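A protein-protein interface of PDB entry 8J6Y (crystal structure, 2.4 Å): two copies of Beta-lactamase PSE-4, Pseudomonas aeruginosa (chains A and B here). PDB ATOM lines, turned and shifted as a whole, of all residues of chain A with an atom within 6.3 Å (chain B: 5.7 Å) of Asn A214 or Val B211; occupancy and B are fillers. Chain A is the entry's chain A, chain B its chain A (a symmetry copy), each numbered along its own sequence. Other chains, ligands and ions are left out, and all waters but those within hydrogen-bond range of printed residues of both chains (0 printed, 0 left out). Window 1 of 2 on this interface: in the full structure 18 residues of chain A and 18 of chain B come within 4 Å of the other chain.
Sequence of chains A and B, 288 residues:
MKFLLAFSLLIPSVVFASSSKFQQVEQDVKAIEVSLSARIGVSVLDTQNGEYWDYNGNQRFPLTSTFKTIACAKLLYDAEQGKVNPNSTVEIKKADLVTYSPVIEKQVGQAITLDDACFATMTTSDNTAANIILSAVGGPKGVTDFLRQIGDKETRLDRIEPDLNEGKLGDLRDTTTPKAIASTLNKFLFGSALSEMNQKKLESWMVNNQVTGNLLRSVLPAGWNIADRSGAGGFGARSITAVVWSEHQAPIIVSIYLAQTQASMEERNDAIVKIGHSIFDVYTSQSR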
ATOM      1  N   GLN A 210     -23.096  18.769  22.532  1.00  0.00           N
ATOM      2  CA  GLN A 210     -21.911  18.873  23.370  1.00  0.00           C
ATOM      3  C   GLN A 210     -21.123  17.573  23.341  1.00  0.00           C
ATOM      4  O   GLN A 210     -20.089  17.470  24.013  1.00  0.00           O
ATOM      5  CB  GLN A 210     -22.273  19.121  24.837  1.00  0.00           C
ATOM      6  CG  GLN A 210     -23.039  20.415  25.070  1.00  0.00           C
ATOM      7  CD  GLN A 210     -22.114  21.593  24.943  1.00  0.00           C
ATOM      8  OE1 GLN A 210     -21.104  21.662  25.635  1.00  0.00           O
ATOM      9  NE2 GLN A 210     -22.455  22.530  24.072  1.00  0.00           N
ATOM     10  N   VAL A 211     -21.617  16.560  22.615  1.00  0.00           N
ATOM     11  CA  VAL A 211     -21.054  15.236  22.830  1.00  0.00           C
ATOM     12  C   VAL A 211     -20.530  14.656  21.530  1.00  0.00           C
ATOM     13  O   VAL A 211     -20.518  13.444  21.418  1.00  0.00           O
ATOM     14  CB  VAL A 211     -22.024  14.269  23.533  1.00  0.00           C
ATOM     15  CG1 VAL A 211     -22.447  14.788  24.917  1.00  0.00           C
ATOM     16  CG2 VAL A 211     -23.227  13.955  22.653  1.00  0.00           C
ATOM     17  N   THR A 212     -20.022  15.506  20.623  1.00  0.00           N
ATOM     18  CA  THR A 212     -19.576  15.041  19.321  1.00  0.00           C
ATOM     19  C   THR A 212     -18.292  15.753  18.889  1.00  0.00           C
ATOM     20  O   THR A 212     -17.837  15.601  17.744  1.00  0.00           O
ATOM     21  CB  THR A 212     -20.651  15.207  18.239  1.00  0.00           C
ATOM     22  OG1 THR A 212     -20.756  16.613  18.073  1.00  0.00           O
ATOM     23  CG2 THR A 212     -21.989  14.560  18.548  1.00  0.00           C
ATOM     24  N   GLY A 213     -17.624  16.413  19.842  1.00  0.00           N
ATOM     25  CA  GLY A 213     -16.378  17.071  19.513  1.00  0.00           C
ATOM     26  C   GLY A 213     -15.344  16.116  18.938  1.00  0.00           C
ATOM     27  O   GLY A 213     -14.408  16.572  18.285  1.00  0.00           O
ATOM     28  N   ASN A 214     -15.488  14.808  19.191  1.00  0.00           N
ATOM     29  CA  ASN A 214     -14.468  13.861  18.763  1.00  0.00           C
ATOM     30  C   ASN A 214     -14.739  13.347  17.348  1.00  0.00           C
ATOM     31  O   ASN A 214     -13.938  12.577  16.814  1.00  0.00           O
ATOM     32  CB  ASN A 214     -14.321  12.700  19.744  1.00  0.00           C
ATOM     33  CG  ASN A 214     -15.581  11.884  19.847  1.00  0.00           C
ATOM     34  OD1 ASN A 214     -16.693  12.389  19.620  1.00  0.00           O
ATOM     35  ND2 ASN A 214     -15.399  10.644  20.280  1.00  0.00           N
ATOM     36  N   LEU A 215     -15.839  13.798  16.732  1.00  0.00           N
ATOM     37  CA  LEU A 215     -16.199  13.309  15.423  1.00  0.00           C
ATOM     38  C   LEU A 215     -15.910  14.393  14.371  1.00  0.00           C
ATOM     39  O   LEU A 215     -14.760  14.818  14.259  1.00  0.00           O
ATOM     40  CB  LEU A 215     -17.643  12.804  15.515  1.00  0.00           C
ATOM     41  CG  LEU A 215     -17.822  11.550  16.381  1.00  0.00           C
ATOM     42  CD1 LEU A 215     -19.231  11.010  16.273  1.00  0.00           C
ATOM     43  CD2 LEU A 215     -16.849  10.454  15.987  1.00  0.00           C
ATOM     44  N   LEU A 216     -16.917  14.806  13.585  1.00  0.00           N
ATOM     45  CA  LEU A 216     -16.703  15.627  12.413  1.00  0.00           C
ATOM     46  C   LEU A 216     -16.223  17.014  12.824  1.00  0.00           C
ATOM     47  O   LEU A 216     -15.364  17.588  12.147  1.00  0.00           O
ATOM     48  CB  LEU A 216     -17.991  15.730  11.595  1.00  0.00           C
ATOM     49  CG  LEU A 216     -18.379  14.497  10.772  1.00  0.00           C
ATOM     50  CD1 LEU A 216     -19.709  14.724  10.016  1.00  0.00           C
ATOM     51  CD2 LEU A 216     -17.257  14.105   9.816  1.00  0.00           C
ATOM     52  N   ARG A 217     -16.735  17.531  13.947  1.00  0.00           N
ATOM     53  CA  ARG A 217     -16.243  18.810  14.453  1.00  0.00           C
ATOM     54  C   ARG A 217     -14.718  18.832  14.567  1.00  0.00           C
ATOM     55  O   ARG A 217     -14.112  19.882  14.421  1.00  0.00           O
ATOM     56  CB  ARG A 217     -16.828  19.120  15.833  1.00  0.00           C
ATOM     57  CG  ARG A 217     -18.304  19.477  15.801  1.00  0.00           C
ATOM     58  CD  ARG A 217     -19.021  19.172  17.101  1.00  0.00           C
ATOM     59  NE  ARG A 217     -20.466  19.327  16.934  1.00  0.00           N
ATOM     60  CZ  ARG A 217     -21.136  20.471  17.040  1.00  0.00           C
ATOM     61  NH1 ARG A 217     -20.481  21.580  17.330  1.00  0.00           N
ATOM     62  NH2 ARG A 217     -22.461  20.487  16.939  1.00  0.00           N
ATOM     63  N   SER A 218     -14.083  17.706  14.899  1.00  0.00           N
ATOM     64  CA  SER A 218     -12.654  17.731  15.139  1.00  0.00           C
ATOM     65  C   SER A 218     -11.879  17.871  13.832  1.00  0.00           C
ATOM     66  O   SER A 218     -10.672  18.069  13.881  1.00  0.00           O
ATOM     67  CB  SER A 218     -12.216  16.521  15.874  1.00  0.00           C
ATOM     68  OG  SER A 218     -12.527  15.357  15.135  1.00  0.00           O
ATOM     69  N   ARG A 238     -21.966   2.586  14.772  1.00  0.00           N
ATOM     70  CA  ARG A 238     -21.466   3.939  15.015  1.00  0.00           C
ATOM     71  C   ARG A 238     -21.917   4.809  13.838  1.00  0.00           C
ATOM     72  O   ARG A 238     -21.839   4.395  12.689  1.00  0.00           O
ATOM     73  CB  ARG A 238     -19.939   3.919  15.139  1.00  0.00           C
ATOM     74  CG  ARG A 238     -19.296   5.217  15.611  1.00  0.00           C
ATOM     75  CD  ARG A 238     -19.373   5.317  17.122  1.00  0.00           C
ATOM     76  NE  ARG A 238     -18.797   6.534  17.659  1.00  0.00           N
ATOM     77  CZ  ARG A 238     -19.471   7.548  18.194  1.00  0.00           C
ATOM     78  NH1 ARG A 238     -20.786   7.638  18.100  1.00  0.00           N
ATOM     79  NH2 ARG A 238     -18.798   8.529  18.755  1.00  0.00           N
ATOM     80  N   MET A 265     -14.312   1.524  20.009  1.00  0.00           N
ATOM     81  CA  MET A 265     -14.898   2.831  19.831  1.00  0.00           C
ATOM     82  C   MET A 265     -13.862   3.772  19.187  1.00  0.00           C
ATOM     83  O   MET A 265     -14.219   4.586  18.353  1.00  0.00           O
ATOM     84  CB  MET A 265     -15.356   3.383  21.184  1.00  0.00           C
ATOM     85  CG  MET A 265     -16.104   4.693  21.122  1.00  0.00           C
ATOM     86  SD  MET A 265     -17.682   4.515  20.249  1.00  0.00           S
ATOM     87  CE  MET A 265     -18.594   3.466  21.373  1.00  0.00           C
ATOM     88  N   ASN A 269     -14.328   5.817  15.876  1.00  0.00           N
ATOM     89  CA  ASN A 269     -14.319   7.276  15.831  1.00  0.00           C
ATOM     90  C   ASN A 269     -13.298   7.735  14.794  1.00  0.00           C
ATOM     91  O   ASN A 269     -13.474   8.754  14.147  1.00  0.00           O
ATOM     92  CB  ASN A 269     -13.950   7.936  17.157  1.00  0.00           C
ATOM     93  CG  ASN A 269     -14.969   7.773  18.253  1.00  0.00           C
ATOM     94  OD1 ASN A 269     -16.169   7.683  18.007  1.00  0.00           O
ATOM     95  ND2 ASN A 269     -14.495   7.767  19.480  1.00  0.00           N
ATOM     96  N   ASP A 270     -12.209   6.985  14.669  1.00  0.00           N
ATOM     97  CA  ASP A 270     -11.137   7.312  13.744  1.00  0.00           C
ATOM     98  C   ASP A 270     -11.625   7.210  12.297  1.00  0.00           C
ATOM     99  O   ASP A 270     -11.319   8.035  11.467  1.00  0.00           O
ATOM    100  CB  ASP A 270      -9.969   6.360  13.980  1.00  0.00           C
ATOM    101  CG  ASP A 270      -8.870   6.462  12.936  1.00  0.00           C
ATOM    102  OD1 ASP A 270      -8.233   7.520  12.844  1.00  0.00           O
ATOM    103  OD2 ASP A 270      -8.670   5.477  12.239  1.00  0.00           O
ATOM    104  N   VAL A 273     -13.693  10.299  11.349  1.00  0.00           N
ATOM    105  CA  VAL A 273     -13.051  11.593  11.133  1.00  0.00           C
ATOM    106  C   VAL A 273     -12.201  11.566   9.861  1.00  0.00           C
ATOM    107  O   VAL A 273     -11.924  12.610   9.271  1.00  0.00           O
ATOM    108  CB  VAL A 273     -12.217  12.058  12.339  1.00  0.00           C
ATOM    109  CG1 VAL A 273     -13.011  11.993  13.629  1.00  0.00           C
ATOM    110  CG2 VAL A 273     -10.943  11.273  12.473  1.00  0.00           C
ATOM    111  N   TYR B 100      -6.555   7.717  15.346  1.00  0.00           N
ATOM    112  CA  TYR B 100      -7.229   8.880  15.905  1.00  0.00           C
ATOM    113  C   TYR B 100      -6.271  10.053  16.130  1.00  0.00           C
ATOM    114  O   TYR B 100      -5.804  10.304  17.244  1.00  0.00           O
ATOM    115  CB  TYR B 100      -8.005   8.589  17.185  1.00  0.00           C
ATOM    116  CG  TYR B 100      -9.015   9.679  17.453  1.00  0.00           C
ATOM    117  CD1 TYR B 100     -10.201   9.767  16.736  1.00  0.00           C
ATOM    118  CD2 TYR B 100      -8.712  10.707  18.319  1.00  0.00           C
ATOM    119  CE1 TYR B 100     -11.070  10.836  16.904  1.00  0.00           C
ATOM    120  CE2 TYR B 100      -9.591  11.754  18.529  1.00  0.00           C
ATOM    121  CZ  TYR B 100     -10.760  11.832  17.811  1.00  0.00           C
ATOM    122  OH  TYR B 100     -11.575  12.890  18.112  1.00  0.00           O
ATOM    123  N   PRO B 102      -7.212  13.548  14.517  1.00  0.00           N
ATOM    124  CA  PRO B 102      -7.979  14.466  13.670  1.00  0.00           C
ATOM    125  C   PRO B 102      -7.203  15.697  13.184  1.00  0.00           C
ATOM    126  O   PRO B 102      -7.269  16.059  12.011  1.00  0.00           O
ATOM    127  CB  PRO B 102      -9.163  14.892  14.557  1.00  0.00           C
ATOM    128  CG  PRO B 102      -8.813  14.426  15.978  1.00  0.00           C
ATOM    129  CD  PRO B 102      -7.822  13.293  15.833  1.00  0.00           C
ATOM    130  N   THR B 123      -7.111  19.195  23.634  1.00  0.00           N
ATOM    131  CA  THR B 123      -8.481  19.575  23.315  1.00  0.00           C
ATOM    132  C   THR B 123      -9.214  18.498  22.498  1.00  0.00           C
ATOM    133  O   THR B 123     -10.444  18.467  22.529  1.00  0.00           O
ATOM    134  CB  THR B 123      -8.539  20.911  22.566  1.00  0.00           C
ATOM    135  OG1 THR B 123      -7.952  20.662  21.292  1.00  0.00           O
ATOM    136  CG2 THR B 123      -7.813  22.027  23.275  1.00  0.00           C
ATOM    137  N   THR B 124      -8.501  17.676  21.707  1.00  0.00           N
ATOM    138  CA  THR B 124      -9.168  16.650  20.904  1.00  0.00           C
ATOM    139  C   THR B 124      -8.668  15.247  21.226  1.00  0.00           C
ATOM    140  O   THR B 124      -9.265  14.257  20.797  1.00  0.00           O
ATOM    141  CB  THR B 124      -8.978  16.839  19.400  1.00  0.00           C
ATOM    142  OG1 THR B 124      -7.612  16.515  19.111  1.00  0.00           O
ATOM    143  CG2 THR B 124      -9.361  18.224  18.917  1.00  0.00           C
ATOM    144  N   SER B 125      -7.527  15.206  21.918  1.00  0.00           N
ATOM    145  CA  SER B 125      -6.838  13.982  22.286  1.00  0.00           C
ATOM    146  C   SER B 125      -6.217  13.310  21.069  1.00  0.00           C
ATOM    147  O   SER B 125      -6.045  12.104  21.089  1.00  0.00           O
ATOM    148  CB  SER B 125      -7.721  13.044  23.041  1.00  0.00           C
ATOM    149  OG  SER B 125      -6.916  12.148  23.759  1.00  0.00           O
ATOM    150  N   ASN B 209     -11.227  21.597  26.423  1.00  0.00           N
ATOM    151  CA  ASN B 209     -11.387  20.203  26.012  1.00  0.00           C
ATOM    152  C   ASN B 209     -12.722  20.041  25.296  1.00  0.00           C
ATOM    153  O   ASN B 209     -13.751  20.424  25.838  1.00  0.00           O
ATOM    154  CB  ASN B 209     -11.330  19.285  27.239  1.00  0.00           C
ATOM    155  CG  ASN B 209     -11.226  17.811  26.924  1.00  0.00           C
ATOM    156  OD1 ASN B 209     -11.580  17.370  25.833  1.00  0.00           O
ATOM    157  ND2 ASN B 209     -10.725  17.045  27.876  1.00  0.00           N
ATOM    158  N   GLN B 210     -12.699  19.477  24.086  1.00  0.00           N
ATOM    159  CA  GLN B 210     -13.887  19.435  23.249  1.00  0.00           C
ATOM    160  C   GLN B 210     -14.487  18.037  23.246  1.00  0.00           C
ATOM    161  O   GLN B 210     -15.497  17.808  22.570  1.00  0.00           O
ATOM    162  CB  GLN B 210     -13.567  19.766  21.789  1.00  0.00           C
ATOM    163  CG  GLN B 210     -12.988  21.159  21.588  1.00  0.00           C
ATOM    164  CD  GLN B 210     -14.068  22.193  21.741  1.00  0.00           C
ATOM    165  OE1 GLN B 210     -15.079  22.137  21.049  1.00  0.00           O
ATOM    166  NE2 GLN B 210     -13.858  23.148  22.635  1.00  0.00           N
ATOM    167  N   VAL B 211     -13.857  17.086  23.949  1.00  0.00           N
ATOM    168  CA  VAL B 211     -14.231  15.702  23.702  1.00  0.00           C
ATOM    169  C   VAL B 211     -14.666  15.025  24.987  1.00  0.00           C
ATOM    170  O   VAL B 211     -14.510  13.820  25.071  1.00  0.00           O
ATOM    171  CB  VAL B 211     -13.137  14.897  22.978  1.00  0.00           C
ATOM    172  CG1 VAL B 211     -12.792  15.502  21.607  1.00  0.00           C
ATOM    173  CG2 VAL B 211     -11.901  14.732  23.853  1.00  0.00           C
ATOM    174  N   THR B 212     -15.286  15.774  25.913  1.00  0.00           N
ATOM    175  CA  THR B 212     -15.660  15.221  27.203  1.00  0.00           C
ATOM    176  C   THR B 212     -17.031  15.737  27.649  1.00  0.00           C
ATOM    177  O   THR B 212     -17.457  15.496  28.789  1.00  0.00           O
ATOM    178  CB  THR B 212     -14.618  15.509  28.291  1.00  0.00           C
ATOM    179  OG1 THR B 212     -14.708  16.912  28.489  1.00  0.00           O
ATOM    180  CG2 THR B 212     -13.204  15.062  27.969  1.00  0.00           C
ATOM    181  N   GLY B 213     -17.786  16.320  26.712  1.00  0.00           N
ATOM    182  CA  GLY B 213     -19.111  16.791  27.054  1.00  0.00           C
ATOM    183  C   GLY B 213     -20.000  15.688  27.604  1.00  0.00           C
ATOM    184  O   GLY B 213     -20.989  15.994  28.266  1.00  0.00           O
ATOM    185  N   ASN B 214     -19.676  14.419  27.321  1.00  0.00           N
ATOM    186  CA  ASN B 214     -20.554  13.330  27.725  1.00  0.00           C
ATOM    187  C   ASN B 214     -20.212  12.825  29.127  1.00  0.00           C
ATOM    188  O   ASN B 214     -20.897  11.938  29.641  1.00  0.00           O
ATOM    189  CB  ASN B 214     -20.541  12.183  26.716  1.00  0.00           C
ATOM    190  CG  ASN B 214     -19.179  11.553  26.595  1.00  0.00           C
ATOM    191  OD1 ASN B 214     -18.148  12.201  26.837  1.00  0.00           O
ATOM    192  ND2 ASN B 214     -19.188  10.310  26.134  1.00  0.00           N
ATOM    193  N   ARG B 229      -9.592  16.095  31.565  1.00  0.00           N
ATOM    194  CA  ARG B 229      -8.820  15.260  30.674  1.00  0.00           C
ATOM    195  C   ARG B 229      -9.315  13.841  30.904  1.00  0.00           C
ATOM    196  O   ARG B 229      -9.383  13.412  32.052  1.00  0.00           O
ATOM    197  CB  ARG B 229      -7.333  15.413  31.000  1.00  0.00           C
ATOM    198  CG  ARG B 229      -6.413  14.552  30.144  1.00  0.00           C
ATOM    199  CD  ARG B 229      -5.854  15.226  28.893  1.00  0.00           C
ATOM    200  NE  ARG B 229      -6.805  15.564  27.843  1.00  0.00           N
ATOM    201  CZ  ARG B 229      -7.240  14.745  26.896  1.00  0.00           C
ATOM    202  NH1 ARG B 229      -6.798  13.509  26.861  1.00  0.00           N
ATOM    203  NH2 ARG B 229      -8.113  15.170  25.987  1.00  0.00           N
ATOM    204  N   SER B 230      -9.682  13.125  29.828  1.00  0.00           N
ATOM    205  CA  SER B 230     -10.336  11.829  29.991  1.00  0.00           C
ATOM    206  C   SER B 230      -9.589  10.759  29.216  1.00  0.00           C
ATOM    207  O   SER B 230      -8.675  11.040  28.451  1.00  0.00           O
ATOM    208  CB  SER B 230     -11.762  11.856  29.576  1.00  0.00           C
ATOM    209  OG  SER B 230     -11.839  11.768  28.173  1.00  0.00           O
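The side-chain carboxylate of Asp A270 lies within hydrogen-bond range of the backbone NH of Tyr B100, 3.0 Å away. The side-chain hydroxyl of Tyr B100 sits at hydrogen-bond distance from the backbone carbonyl oxygen of Asn A214, at 2.7 Å.
O of Leu A215 sits at hydrogen-bond distance from OG of Ser A218 (2.5 Å). The side-chain amide nitrogen of Asn A214 sits close to the side-chain amide nitrogen of Asn A269 (3.1 Å). The backbone carbonyl oxygen (O) of Thr B123 is in hydrogen-bond range of the backbone NH (N) of Gln B210 (2.9 Å). The side-chain amide oxygen of Asn B209 sits at hydrogen-bond distance from the backbone NH of Val B211.
Among the printed residues, merely in contact across the chains: Gly A213 with Gln B210, Gln A210 with Gly B213, Ser A218 with Pro B102, Asn A214 with Val B211, Val A211 with Asn B214, Gly A213 with Val B211, Val A211 with Gly B213, Val A273 with Tyr B100 and Ser A218 with Tyr B100.
Printed residues of chain B within 4 Å of Gln A210: Gly B213 (3.3 Å). Asn A214 touches just these residues of chain B: Tyr B100 (2.7 Å) and Val B211 (3.7 Å). Of the printed residues of chain B, Val A273 touches Tyr B100. Of the printed residues of chain A, Tyr B100 touches Asn A214, Ser A218, Asp A270 and Val A273. Of the printed residues of chain A, Pro B102 touches Ser A218. Thr B123 touches none of the printed residues of chain A. Of chain A, only Gly A213 and Asn A214 come within 4 Å of Val B211. The nearest printed residue of chain B that does not touch Gln A210 is Asn B214 (4.5 Å).
Of the 13 printed residues of chain B, 6 touch a printed residue of chain A. Hydrophobic or aromatic side chains of chain B that line the printed part of chain A: Tyr B100, Pro B102 and Val B211. Hydrophobic or aromatic side chains of chain A within 4 Å of the printed part of chain B: Val A211 and Val A273. Among the printed residues, no Asp or Glu carboxylate lies within 4 Å of a Lys or Arg side-chain nitrogen of the other chain.
Gln A210 touches Gly B213, and with the chains exchanged Gly A213 touches Gln B210. Val A211 touches Gly B213, and with the chains exchanged Gly A213 touches Val B211. Val A211 touches Asn B214, and with the chains exchanged Asn A214 touches Val B211. Positions printed for both chains: 210, 211, 212, 213 and 214. Of the 11 pairs that touch across the chains among the printed residues, 6 have their exchanged pair printed and touching as well.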
